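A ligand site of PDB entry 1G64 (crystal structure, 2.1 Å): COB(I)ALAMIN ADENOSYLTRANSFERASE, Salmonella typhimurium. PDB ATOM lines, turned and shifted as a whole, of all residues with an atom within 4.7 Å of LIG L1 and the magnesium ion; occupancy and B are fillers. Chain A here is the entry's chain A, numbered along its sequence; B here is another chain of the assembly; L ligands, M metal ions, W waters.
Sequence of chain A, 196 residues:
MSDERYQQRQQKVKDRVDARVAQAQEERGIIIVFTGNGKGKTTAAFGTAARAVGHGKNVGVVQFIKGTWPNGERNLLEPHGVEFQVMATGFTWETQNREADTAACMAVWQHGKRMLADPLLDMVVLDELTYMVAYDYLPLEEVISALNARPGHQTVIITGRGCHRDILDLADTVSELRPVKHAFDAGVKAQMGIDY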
ATOM      1  N   ASN A  37     -15.408  21.945 -18.080  1.00  0.00           N
ATOM      2  CA  ASN A  37     -14.165  21.605 -18.768  1.00  0.00           C
ATOM      3  C   ASN A  37     -13.039  22.607 -18.700  1.00  0.00           C
ATOM      4  O   ASN A  37     -11.898  22.284 -19.022  1.00  0.00           O
ATOM      5  CB  ASN A  37     -14.416  21.311 -20.250  1.00  0.00           C
ATOM      6  CG  ASN A  37     -14.955  19.929 -20.473  1.00  0.00           C
ATOM      7  OD1 ASN A  37     -14.820  19.412 -21.587  1.00  0.00           O
ATOM      8  ND2 ASN A  37     -15.511  19.340 -19.430  1.00  0.00           N
ATOM      9  N   GLY A  38     -13.334  23.853 -18.342  1.00  0.00           N
ATOM     10  CA  GLY A  38     -12.242  24.834 -18.236  1.00  0.00           C
ATOM     11  C   GLY A  38     -11.339  24.571 -16.994  1.00  0.00           C
ATOM     12  O   GLY A  38     -11.791  24.017 -15.963  1.00  0.00           O
ATOM     13  N   LYS A  39     -10.067  24.971 -17.126  1.00  0.00           N
ATOM     14  CA  LYS A  39      -9.020  24.869 -16.106  1.00  0.00           C
ATOM     15  C   LYS A  39      -9.393  25.675 -14.893  1.00  0.00           C
ATOM     16  O   LYS A  39      -9.897  26.782 -15.094  1.00  0.00           O
ATOM     17  CB  LYS A  39      -7.794  25.577 -16.698  1.00  0.00           C
ATOM     18  CG  LYS A  39      -6.803  26.104 -15.683  1.00  0.00           C
ATOM     19  CD  LYS A  39      -5.447  26.707 -16.224  1.00  0.00           C
ATOM     20  CE  LYS A  39      -4.159  26.421 -15.349  1.00  0.00           C
ATOM     21  NZ  LYS A  39      -4.341  25.879 -13.931  1.00  0.00           N
ATOM     22  N   GLY A  40      -9.249  25.161 -13.658  1.00  0.00           N
ATOM     23  CA  GLY A  40      -9.559  26.058 -12.532  1.00  0.00           C
ATOM     24  C   GLY A  40     -10.359  25.490 -11.413  1.00  0.00           C
ATOM     25  O   GLY A  40     -10.721  26.203 -10.467  1.00  0.00           O
ATOM     26  N   LYS A  41     -10.659  24.244 -11.470  1.00  0.00           N
ATOM     27  CA  LYS A  41     -11.522  23.711 -10.400  1.00  0.00           C
ATOM     28  C   LYS A  41     -10.737  23.369  -9.101  1.00  0.00           C
ATOM     29  O   LYS A  41     -11.156  23.708  -7.967  1.00  0.00           O
ATOM     30  CB  LYS A  41     -12.285  22.432 -10.854  1.00  0.00           C
ATOM     31  CG  LYS A  41     -13.296  22.497 -12.003  1.00  0.00           C
ATOM     32  CD  LYS A  41     -13.103  21.339 -12.996  1.00  0.00           C
ATOM     33  CE  LYS A  41     -12.313  21.843 -14.208  1.00  0.00           C
ATOM     34  NZ  LYS A  41     -11.818  20.736 -15.014  1.00  0.00           N
ATOM     35  N   THR A  42      -9.650  22.601  -9.328  1.00  0.00           N
ATOM     36  CA  THR A  42      -8.730  22.202  -8.327  1.00  0.00           C
ATOM     37  C   THR A  42      -8.074  23.509  -7.816  1.00  0.00           C
ATOM     38  O   THR A  42      -8.011  23.801  -6.619  1.00  0.00           O
ATOM     39  CB  THR A  42      -7.767  21.268  -8.998  1.00  0.00           C
ATOM     40  OG1 THR A  42      -8.539  20.097  -9.128  1.00  0.00           O
ATOM     41  CG2 THR A  42      -6.568  21.038  -8.070  1.00  0.00           C
ATOM     42  N   THR A  43      -7.645  24.353  -8.765  1.00  0.00           N
ATOM     43  CA  THR A  43      -7.076  25.624  -8.381  1.00  0.00           C
ATOM     44  C   THR A  43      -7.950  26.426  -7.449  1.00  0.00           C
ATOM     45  O   THR A  43      -7.503  26.972  -6.457  1.00  0.00           O
ATOM     46  CB  THR A  43      -6.315  26.404  -9.459  1.00  0.00           C
ATOM     47  OG1 THR A  43      -7.058  26.471 -10.652  1.00  0.00           O
ATOM     48  CG2 THR A  43      -4.955  25.743  -9.735  1.00  0.00           C
ATOM     49  N   ASP A 127     -10.892  16.391  -3.755  1.00  0.00           N
ATOM     50  CA  ASP A 127     -10.413  16.582  -5.095  1.00  0.00           C
ATOM     51  C   ASP A 127     -10.571  15.422  -6.042  1.00  0.00           C
ATOM     52  O   ASP A 127     -10.005  14.337  -5.852  1.00  0.00           O
ATOM     53  CB  ASP A 127      -8.950  17.055  -4.977  1.00  0.00           C
ATOM     54  CG  ASP A 127      -8.397  17.749  -6.166  1.00  0.00           C
ATOM     55  OD1 ASP A 127      -7.340  17.446  -6.650  1.00  0.00           O
ATOM     56  OD2 ASP A 127      -9.158  18.698  -6.617  1.00  0.00           O
ATOM     57  N   GLU A 128     -11.374  15.737  -7.052  1.00  0.00           N
ATOM     58  CA  GLU A 128     -11.716  14.879  -8.156  1.00  0.00           C
ATOM     59  C   GLU A 128     -12.547  13.669  -7.863  1.00  0.00           C
ATOM     60  O   GLU A 128     -12.413  12.619  -8.462  1.00  0.00           O
ATOM     61  CB  GLU A 128     -10.534  14.609  -9.032  1.00  0.00           C
ATOM     62  CG  GLU A 128     -10.370  15.863  -9.916  1.00  0.00           C
ATOM     63  CD  GLU A 128      -8.940  16.102  -9.818  1.00  0.00           C
ATOM     64  OE1 GLU A 128      -8.269  15.267  -9.239  1.00  0.00           O
ATOM     65  OE2 GLU A 128      -8.548  17.246 -10.326  1.00  0.00           O
ATOM     66  N   TYR A 131     -15.129  11.757 -10.772  1.00  0.00           N
ATOM     67  CA  TYR A 131     -14.906  10.558 -11.529  1.00  0.00           C
ATOM     68  C   TYR A 131     -14.989   9.340 -10.676  1.00  0.00           C
ATOM     69  O   TYR A 131     -15.157   8.212 -11.119  1.00  0.00           O
ATOM     70  CB  TYR A 131     -13.533  10.587 -12.157  1.00  0.00           C
ATOM     71  CG  TYR A 131     -13.247  11.899 -12.818  1.00  0.00           C
ATOM     72  CD1 TYR A 131     -12.578  12.897 -12.123  1.00  0.00           C
ATOM     73  CD2 TYR A 131     -13.589  12.150 -14.145  1.00  0.00           C
ATOM     74  CE1 TYR A 131     -12.278  14.124 -12.695  1.00  0.00           C
ATOM     75  CE2 TYR A 131     -13.251  13.349 -14.758  1.00  0.00           C
ATOM     76  CZ  TYR A 131     -12.637  14.361 -14.018  1.00  0.00           C
ATOM     77  OH  TYR A 131     -12.316  15.575 -14.551  1.00  0.00           O
ATOM     78  N   THR A 159     -14.546  18.776  -6.464  1.00  0.00           N
ATOM     79  CA  THR A 159     -14.202  19.193  -7.792  1.00  0.00           C
ATOM     80  C   THR A 159     -14.140  18.005  -8.713  1.00  0.00           C
ATOM     81  O   THR A 159     -14.055  16.856  -8.242  1.00  0.00           O
ATOM     82  CB  THR A 159     -12.853  19.904  -7.893  1.00  0.00           C
ATOM     83  OG1 THR A 159     -11.835  18.960  -7.982  1.00  0.00           O
ATOM     84  CG2 THR A 159     -12.609  20.706  -6.649  1.00  0.00           C
ATOM     85  N   ARG A 161     -14.661  17.066 -13.385  1.00  0.00           N
ATOM     86  CA  ARG A 161     -15.559  16.962 -14.508  1.00  0.00           C
ATOM     87  C   ARG A 161     -16.636  15.935 -14.227  1.00  0.00           C
ATOM     88  O   ARG A 161     -16.370  14.850 -13.718  1.00  0.00           O
ATOM     89  CB  ARG A 161     -14.872  16.553 -15.819  1.00  0.00           C
ATOM     90  CG  ARG A 161     -14.271  17.688 -16.604  1.00  0.00           C
ATOM     91  CD  ARG A 161     -13.307  17.232 -17.714  1.00  0.00           C
ATOM     92  NE  ARG A 161     -12.570  18.362 -18.291  1.00  0.00           N
ATOM     93  CZ  ARG A 161     -12.141  18.440 -19.561  1.00  0.00           C
ATOM     94  NH1 ARG A 161     -12.340  17.499 -20.479  1.00  0.00           N
ATOM     95  NH2 ARG A 161     -11.468  19.494 -19.901  1.00  0.00           N
ATOM     96  N   HIS A 182      -8.243  27.922 -23.877  1.00  0.00           N
ATOM     97  CA  HIS A 182      -7.214  27.139 -23.232  1.00  0.00           C
ATOM     98  C   HIS A 182      -5.882  27.040 -23.993  1.00  0.00           C
ATOM     99  O   HIS A 182      -5.828  26.488 -25.093  1.00  0.00           O
ATOM    100  CB  HIS A 182      -7.695  25.769 -22.728  1.00  0.00           C
ATOM    101  CG  HIS A 182      -6.642  25.142 -21.873  1.00  0.00           C
ATOM    102  ND1 HIS A 182      -5.446  24.684 -22.403  1.00  0.00           N
ATOM    103  CD2 HIS A 182      -6.627  24.954 -20.527  1.00  0.00           C
ATOM    104  CE1 HIS A 182      -4.756  24.220 -21.370  1.00  0.00           C
ATOM    105  NE2 HIS A 182      -5.444  24.381 -20.220  1.00  0.00           N
ATOM    106  N   PHE A 184      -3.280  25.296 -24.098  1.00  0.00           N
ATOM    107  CA  PHE A 184      -2.855  24.077 -24.720  1.00  0.00           C
ATOM    108  C   PHE A 184      -3.413  23.895 -26.116  1.00  0.00           C
ATOM    109  O   PHE A 184      -2.918  23.100 -26.925  1.00  0.00           O
ATOM    110  CB  PHE A 184      -3.357  22.928 -23.865  1.00  0.00           C
ATOM    111  CG  PHE A 184      -2.917  21.618 -24.444  1.00  0.00           C
ATOM    112  CD1 PHE A 184      -1.593  21.207 -24.326  1.00  0.00           C
ATOM    113  CD2 PHE A 184      -3.799  20.817 -25.159  1.00  0.00           C
ATOM    114  CE1 PHE A 184      -1.182  19.975 -24.827  1.00  0.00           C
ATOM    115  CE2 PHE A 184      -3.401  19.585 -25.692  1.00  0.00           C
ATOM    116  CZ  PHE A 184      -2.085  19.160 -25.504  1.00  0.00           C
ATOM    117  N   ILE A 194       1.923  26.438 -13.421  1.00  0.00           N
ATOM    118  CA  ILE A 194       0.609  26.803 -13.968  1.00  0.00           C
ATOM    119  C   ILE A 194      -0.335  25.633 -13.967  1.00  0.00           C
ATOM    120  O   ILE A 194      -1.424  25.710 -13.416  1.00  0.00           O
ATOM    121  CB  ILE A 194       0.766  27.317 -15.389  1.00  0.00           C
ATOM    122  CG1 ILE A 194       1.836  28.403 -15.409  1.00  0.00           C
ATOM    123  CG2 ILE A 194      -0.533  27.917 -15.895  1.00  0.00           C
ATOM    124  CD1 ILE A 194       2.961  28.167 -16.460  1.00  0.00           C
ATOM    125  N   ASP A 195       0.143  24.570 -14.561  1.00  0.00           N
ATOM    126  CA  ASP A 195      -0.584  23.357 -14.726  1.00  0.00           C
ATOM    127  C   ASP A 195      -0.522  22.304 -13.677  1.00  0.00           C
ATOM    128  O   ASP A 195      -1.510  21.608 -13.499  1.00  0.00           O
ATOM    129  CB  ASP A 195      -0.303  22.768 -16.108  1.00  0.00           C
ATOM    130  CG  ASP A 195      -0.408  23.836 -17.139  1.00  0.00           C
ATOM    131  OD1 ASP A 195      -1.452  24.317 -17.539  1.00  0.00           O
ATOM    132  OD2 ASP A 195       0.786  24.227 -17.483  1.00  0.00           O
ATOM    133  N   ARG B  51       0.023  27.182  -5.970  1.00  0.00           N
ATOM    134  CA  ARG B  51       0.587  26.034  -6.658  1.00  0.00           C
ATOM    135  C   ARG B  51       2.037  26.340  -7.151  1.00  0.00           C
ATOM    136  O   ARG B  51       2.989  25.517  -7.137  1.00  0.00           O
ATOM    137  CB  ARG B  51      -0.346  25.845  -7.831  1.00  0.00           C
ATOM    138  CG  ARG B  51       0.293  24.992  -8.889  1.00  0.00           C
ATOM    139  CD  ARG B  51      -0.701  24.648  -9.964  1.00  0.00           C
ATOM    140  NE  ARG B  51      -1.699  23.657  -9.546  1.00  0.00           N
ATOM    141  CZ  ARG B  51      -2.592  23.082 -10.386  1.00  0.00           C
ATOM    142  NH1 ARG B  51      -2.684  23.327 -11.707  1.00  0.00           N
ATOM    143  NH2 ARG B  51      -3.448  22.219  -9.860  1.00  0.00           N
HETATM  144  P1  LIG L   1      -6.352  23.017 -12.487  1.00  0.00           P
HETATM  145  O1  LIG L   1      -5.916  22.057 -11.436  1.00  0.00           O
HETATM  146  O2  LIG L   1      -7.167  24.008 -11.817  1.00  0.00           O
HETATM  147  O3  LIG L   1      -5.233  23.752 -13.215  1.00  0.00           O
HETATM  148  P2  LIG L   1      -8.742  21.666 -13.180  1.00  0.00           P
HETATM  149  O4  LIG L   1      -9.671  22.770 -13.535  1.00  0.00           O
HETATM  150  O5  LIG L   1      -9.030  21.108 -11.838  1.00  0.00           O
HETATM  151  O6  LIG L   1      -7.259  22.151 -13.368  1.00  0.00           O
HETATM  152  P3  LIG L   1      -8.510  18.979 -14.304  1.00  0.00           P
HETATM  153  O7  LIG L   1      -9.032  18.233 -15.494  1.00  0.00           O
HETATM  154  O8  LIG L   1      -8.803  18.315 -13.014  1.00  0.00           O
HETATM  155  O9  LIG L   1      -8.802  20.512 -14.296  1.00  0.00           O
HETATM  156  O10 LIG L   1      -6.959  19.139 -14.563  1.00  0.00           O
HETATM  157  C1  LIG L   1      -6.130  18.030 -14.888  1.00  0.00           C
HETATM  158  C2  LIG L   1      -4.933  18.602 -15.611  1.00  0.00           C
HETATM  159  O11 LIG L   1      -5.417  19.080 -16.857  1.00  0.00           O
HETATM  160  C3  LIG L   1      -4.303  19.840 -15.009  1.00  0.00           C
HETATM  161  O12 LIG L   1      -2.886  19.829 -15.313  1.00  0.00           O
HETATM  162  C4  LIG L   1      -4.988  20.837 -15.516  1.00  0.00           C
HETATM  163  O13 LIG L   1      -4.349  22.107 -15.373  1.00  0.00           O
HETATM  164  C5  LIG L   1      -5.208  20.466 -16.940  1.00  0.00           C
HETATM  165  N1  LIG L   1      -6.391  20.966 -17.531  1.00  0.00           N
HETATM  166  C6  LIG L   1      -7.526  21.362 -16.918  1.00  0.00           C
HETATM  167  N2  LIG L   1      -8.416  21.826 -17.788  1.00  0.00           N
HETATM  168  C7  LIG L   1      -7.810  21.693 -19.012  1.00  0.00           C
HETATM  169  C8  LIG L   1      -8.275  22.021 -20.307  1.00  0.00           C
HETATM  170  N3  LIG L   1      -9.514  22.538 -20.492  1.00  0.00           N
HETATM  171  N4  LIG L   1      -7.395  21.770 -21.312  1.00  0.00           N
HETATM  172  C9  LIG L   1      -6.153  21.240 -21.010  1.00  0.00           C
HETATM  173  N5  LIG L   1      -5.648  20.897 -19.850  1.00  0.00           N
HETATM  174  C10 LIG L   1      -6.553  21.140 -18.877  1.00  0.00           C
HETATM  175 CO1  LG2 L   2      -6.177  12.866 -18.139  1.00  0.00          CO
HETATM  176  N1  LG2 L   2      -4.551  13.143 -18.931  1.00  0.00           N
HETATM  177  N2  LG2 L   2      -5.547  11.255 -17.386  1.00  0.00           N
HETATM  178  N3  LG2 L   2      -7.986  12.580 -17.636  1.00  0.00           N
HETATM  179  N4  LG2 L   2      -6.652  14.407 -19.019  1.00  0.00           N
HETATM  180  C1  LG2 L   2      -4.469  14.225 -19.946  1.00  0.00           C
HETATM  181  C2  LG2 L   2      -4.834  13.712 -21.329  1.00  0.00           C
HETATM  182  C3  LG2 L   2      -2.899  14.685 -19.827  1.00  0.00           C
HETATM  183  C4  LG2 L   2      -2.332  15.159 -21.164  1.00  0.00           C
HETATM  184  C5  LG2 L   2      -2.765  15.768 -18.778  1.00  0.00           C
HETATM  185  C6  LG2 L   2      -1.356  16.122 -18.433  1.00  0.00           C
HETATM  186  O1  LG2 L   2      -0.610  16.728 -19.209  1.00  0.00           O
HETATM  187  N5  LG2 L   2      -0.927  15.665 -17.246  1.00  0.00           N
HETATM  188  C7  LG2 L   2      -2.257  13.412 -19.255  1.00  0.00           C
HETATM  189  C8  LG2 L   2      -1.637  12.354 -20.186  1.00  0.00           C
HETATM  190  C9  LG2 L   2      -0.093  12.451 -20.347  1.00  0.00           C
HETATM  191  C10 LG2 L   2       0.461  11.794 -21.597  1.00  0.00           C
HETATM  192  O2  LG2 L   2      -0.042  10.728 -22.028  1.00  0.00           O
HETATM  193  N6  LG2 L   2       1.510  12.338 -22.186  1.00  0.00           N
HETATM  194  C11 LG2 L   2      -3.370  12.847 -18.447  1.00  0.00           C
HETATM  195  C12 LG2 L   2      -3.172  11.794 -17.504  1.00  0.00           C
HETATM  196  C13 LG2 L   2      -1.687  11.427 -17.221  1.00  0.00           C
HETATM  197  C14 LG2 L   2      -4.168  10.972 -17.180  1.00  0.00           C
HETATM  198  C15 LG2 L   2      -4.120   9.869 -16.115  1.00  0.00           C
HETATM  199  C16 LG2 L   2      -2.918   8.905 -16.199  1.00  0.00           C
HETATM  200  C17 LG2 L   2      -4.187  10.614 -14.750  1.00  0.00           C
HETATM  201  C18 LG2 L   2      -3.677   9.761 -13.603  1.00  0.00           C
HETATM  202  O3  LG2 L   2      -4.215   8.686 -13.322  1.00  0.00           O
HETATM  203  N7  LG2 L   2      -2.633  10.229 -12.959  1.00  0.00           N
HETATM  204  C19 LG2 L   2      -5.497   9.176 -16.372  1.00  0.00           C
HETATM  205  C20 LG2 L   2      -5.477   8.052 -17.397  1.00  0.00           C
HETATM  206  C21 LG2 L   2      -6.729   7.772 -18.201  1.00  0.00           C
HETATM  207  C22 LG2 L   2      -6.372   7.100 -19.456  1.00  0.00           C
HETATM  208  O4  LG2 L   2      -5.255   6.623 -19.629  1.00  0.00           O
HETATM  209  N8  LG2 L   2      -7.282   7.033 -20.447  1.00  0.00           N
HETATM  210  C23 LG2 L   2      -6.305  10.358 -16.818  1.00  0.00           C
HETATM  211  C24 LG2 L   2      -7.632  10.482 -16.511  1.00  0.00           C
HETATM  212  C25 LG2 L   2      -8.411  11.429 -17.092  1.00  0.00           C
HETATM  213  C26 LG2 L   2      -9.811  11.596 -16.660  1.00  0.00           C
HETATM  214  C27 LG2 L   2     -10.520  10.200 -16.694  1.00  0.00           C
HETATM  215  C28 LG2 L   2      -9.727  12.101 -15.234  1.00  0.00           C
HETATM  216  C29 LG2 L   2     -10.322  12.684 -17.570  1.00  0.00           C
HETATM  217  C30 LG2 L   2     -11.019  12.262 -18.882  1.00  0.00           C
HETATM  218  C31 LG2 L   2     -12.540  11.889 -18.804  1.00  0.00           C
HETATM  219  C32 LG2 L   2     -13.429  13.102 -18.638  1.00  0.00           C
HETATM  220  O5  LG2 L   2     -14.281  13.113 -17.721  1.00  0.00           O
HETATM  221  N9  LG2 L   2     -13.346  14.094 -19.547  1.00  0.00           N
HETATM  222  C33 LG2 L   2      -9.033  13.337 -17.992  1.00  0.00           C
HETATM  223  C34 LG2 L   2      -8.917  14.613 -18.509  1.00  0.00           C
HETATM  224  C35 LG2 L   2     -10.066  15.565 -18.320  1.00  0.00           C
HETATM  225  C36 LG2 L   2      -7.688  15.174 -18.879  1.00  0.00           C
HETATM  226  C37 LG2 L   2      -7.556  16.378 -19.726  1.00  0.00           C
HETATM  227  C38 LG2 L   2      -7.559  17.573 -18.781  1.00  0.00           C
HETATM  228  C39 LG2 L   2      -8.603  16.586 -20.793  1.00  0.00           C
HETATM  229  C40 LG2 L   2      -8.683  15.595 -21.918  1.00  0.00           C
HETATM  230  C41 LG2 L   2      -9.775  16.008 -22.847  1.00  0.00           C
HETATM  231  O6  LG2 L   2     -10.930  16.141 -22.374  1.00  0.00           O
HETATM  232  N10 LG2 L   2      -9.400  16.341 -24.089  1.00  0.00           N
HETATM  233  C42 LG2 L   2      -6.180  16.195 -20.370  1.00  0.00           C
HETATM  234  C43 LG2 L   2      -5.401  17.464 -20.443  1.00  0.00           C
HETATM  235  C44 LG2 L   2      -4.758  17.676 -21.817  1.00  0.00           C
HETATM  236  O7  LG2 L   2      -5.073  16.947 -22.744  1.00  0.00           O
HETATM  237  N11 LG2 L   2      -3.900  18.697 -21.884  1.00  0.00           N
HETATM  238  C45 LG2 L   2      -5.537  15.200 -19.445  1.00  0.00           C
HETATM  239  C46 LG2 L   2     -10.290  16.803 -25.168  1.00  0.00           C
HETATM  240  C47 LG2 L   2     -11.074  15.671 -25.824  1.00  0.00           C
HETATM  241  C48 LG2 L   2     -12.106  16.247 -26.821  1.00  0.00           C
HETATM  242  O8  LG2 L   2     -10.113  14.927 -26.659  1.00  0.00           O
HETATM  243  O9  LG2 L   2     -11.156  12.615 -26.924  1.00  0.00           O
HETATM  244  O10 LG2 L   2      -8.659  13.083 -27.236  1.00  0.00           O
HETATM  245  P1  LG2 L   2      -9.924  13.366 -26.492  1.00  0.00           P
HETATM  246  O11 LG2 L   2      -9.708  13.229 -24.937  1.00  0.00           O
HETATM  247  C49 LG2 L   2      -9.747  11.925 -24.311  1.00  0.00           C
HETATM  248  C50 LG2 L   2      -8.412  11.546 -23.726  1.00  0.00           C
HETATM  249  O12 LG2 L   2      -7.738  12.740 -23.218  1.00  0.00           O
HETATM  250  C51 LG2 L   2      -8.898  10.626 -22.534  1.00  0.00           C
HETATM  251  O13 LG2 L   2     -10.045  11.303 -22.046  1.00  0.00           O
HETATM  252  C52 LG2 L   2     -10.696  12.007 -23.139  1.00  0.00           C
HETATM  253  C53 LG2 L   2     -12.024  11.265 -23.419  1.00  0.00           C
HETATM  254  O14 LG2 L   2     -11.807   9.918 -24.018  1.00  0.00           O
HETATM  255  N12 LG2 L   2      -7.955  10.567 -21.398  1.00  0.00           N
HETATM  256  C54 LG2 L   2      -6.682   9.893 -21.430  1.00  0.00           C
HETATM  257  C55 LG2 L   2      -7.852  11.493 -20.433  1.00  0.00           C
HETATM  258  N13 LG2 L   2      -6.629  11.594 -19.894  1.00  0.00           N
HETATM  259  C56 LG2 L   2      -5.893  10.595 -20.550  1.00  0.00           C
HETATM  260  C57 LG2 L   2      -4.530  10.205 -20.386  1.00  0.00           C
HETATM  261  C58 LG2 L   2      -4.077   9.148 -21.146  1.00  0.00           C
HETATM  262  C59 LG2 L   2      -2.620   8.710 -20.965  1.00  0.00           C
HETATM  263  C60 LG2 L   2      -4.892   8.502 -22.087  1.00  0.00           C
HETATM  264  C61 LG2 L   2      -4.330   7.388 -22.937  1.00  0.00           C
HETATM  265  C62 LG2 L   2      -6.241   8.849 -22.237  1.00  0.00           C
HETATM  266 MG    MG M   1      -8.436  19.222 -10.936  1.00  0.00          MG
HETATM  267  O   HOH W   1      -6.411  19.792 -11.474  1.00  0.00           O
HETATM  268  O   HOH W   2      -4.048  23.720 -17.429  1.00  0.00           O
HETATM  269  O   HOH W   3     -10.632  18.912 -10.467  1.00  0.00           O
HETATM  270  O   HOH W   4      -1.041  17.092 -14.356  1.00  0.00           O
HETATM  271  O   HOH W   5     -10.816  22.739 -23.397  1.00  0.00           O
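N of Thr 42 sits close to O5 of LIG L1, 3.0 Å away.
The side-chain amino group (NZ) of Lys 39 lies within salt-bridge range of an oxygen (O3) of LIG L1, 2.4 Å away.
O4 of LIG L1 is in hydrogen-bond range of N of Gly 40 (2.4 Å).
The backbone NH (N) of Lys 41 sits at hydrogen-bond distance from an oxygen (O4) of LIG L1, 2.7 Å away.
O4 of LIG L1 is in salt-bridge range of NZ of Lys 41, 3.3 Å away.
N of Thr 43 sits at hydrogen-bond distance from O2 of LIG L1 (3.1 Å).
O2 of LIG L1 is in hydrogen-bond range of OG1 of Thr 43, at 2.7 Å.
O of Asn 37 lies within hydrogen-bond range of N3 of LIG L1, 2.8 Å away.
The backbone carbonyl oxygen (O) of Asp 195 lies within hydrogen-bond range of an oxygen (O12) of LIG L1 (2.9 Å).
NH2 of Arg 51 of chain B lies within salt-bridge range of O1 of LIG L1, at 2.9 Å.
A ring nitrogen (NE2) of His 182 lies close to a nitrogen (N4) of LIG L1 (3.4 Å).
NH1 of Arg 161 lies within hydrogen-bond range of O6 of LG2 L2 (2.7 Å).
A nitrogen (N5) of LIG L1 is in hydrogen-bond range of a nitrogen (N11) of LG2 L2.
OD2 of Asp 127 sits close to OG1 of Thr 42 (2.9 Å).
O of Thr 159 sits close to N of Glu 128 (3.1 Å).
The side-chain amino group (NZ) of Lys 39 sits at hydrogen-bond distance from the backbone carbonyl oxygen (O) of Ile 194 (3.0 Å).
The side-chain amino group of Lys 41 lies close to the backbone carbonyl oxygen of Gly 38, at 3.4 Å.
O of Asn 37 sits at hydrogen-bond distance from NH2 of Arg 161 (3.0 Å).
The backbone carbonyl oxygen (O) of Asp 195 lies within hydrogen-bond range of the guanidinium group (NH1) of Arg 51 of chain B (2.7 Å).
The guanidinium group of Arg 51 of chain B is in hydrogen-bond range of the backbone carbonyl oxygen of Ile 194, at 3.2 Å.
N of Arg 161 is in hydrogen-bond range of OH of Tyr 131.
An oxygen (O4) of LIG L1 sits close to the backbone carbonyl oxygen (O) of Gly 38 (3.5 Å).
Arg 161 touches LIG L1.
Of the 17 residues printed, 12 come within 4 Å of LIG L1.
The nearest printed residue that does not touch the magnesium ion is Asp 127 (4.4 Å).
The magnesium ion is bound by the side-chain hydroxyl (OG1) of Thr 42 (2.0 Å), the side-chain carboxylate (OE2) of Glu 128 (2.1 Å), water W1 (2.2 Å), an oxygen (O5) of LIG L1 (2.2 Å), water W3 (2.3 Å) and an oxygen (O8) of LIG L1 (2.3 Å).
The magnesium ion has six donor atoms within binding distance.
Water W2 lies within hydrogen-bond range of O13 of LIG L1 (2.6 Å), OD1 of Asp 195 (2.7 Å) and NE2 of His 182 (3.2 Å).
Water W4 bridges a nitrogen (N5) of LG2 L2 (3.2 Å) and an oxygen (O12) of LIG L1 (3.4 Å).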
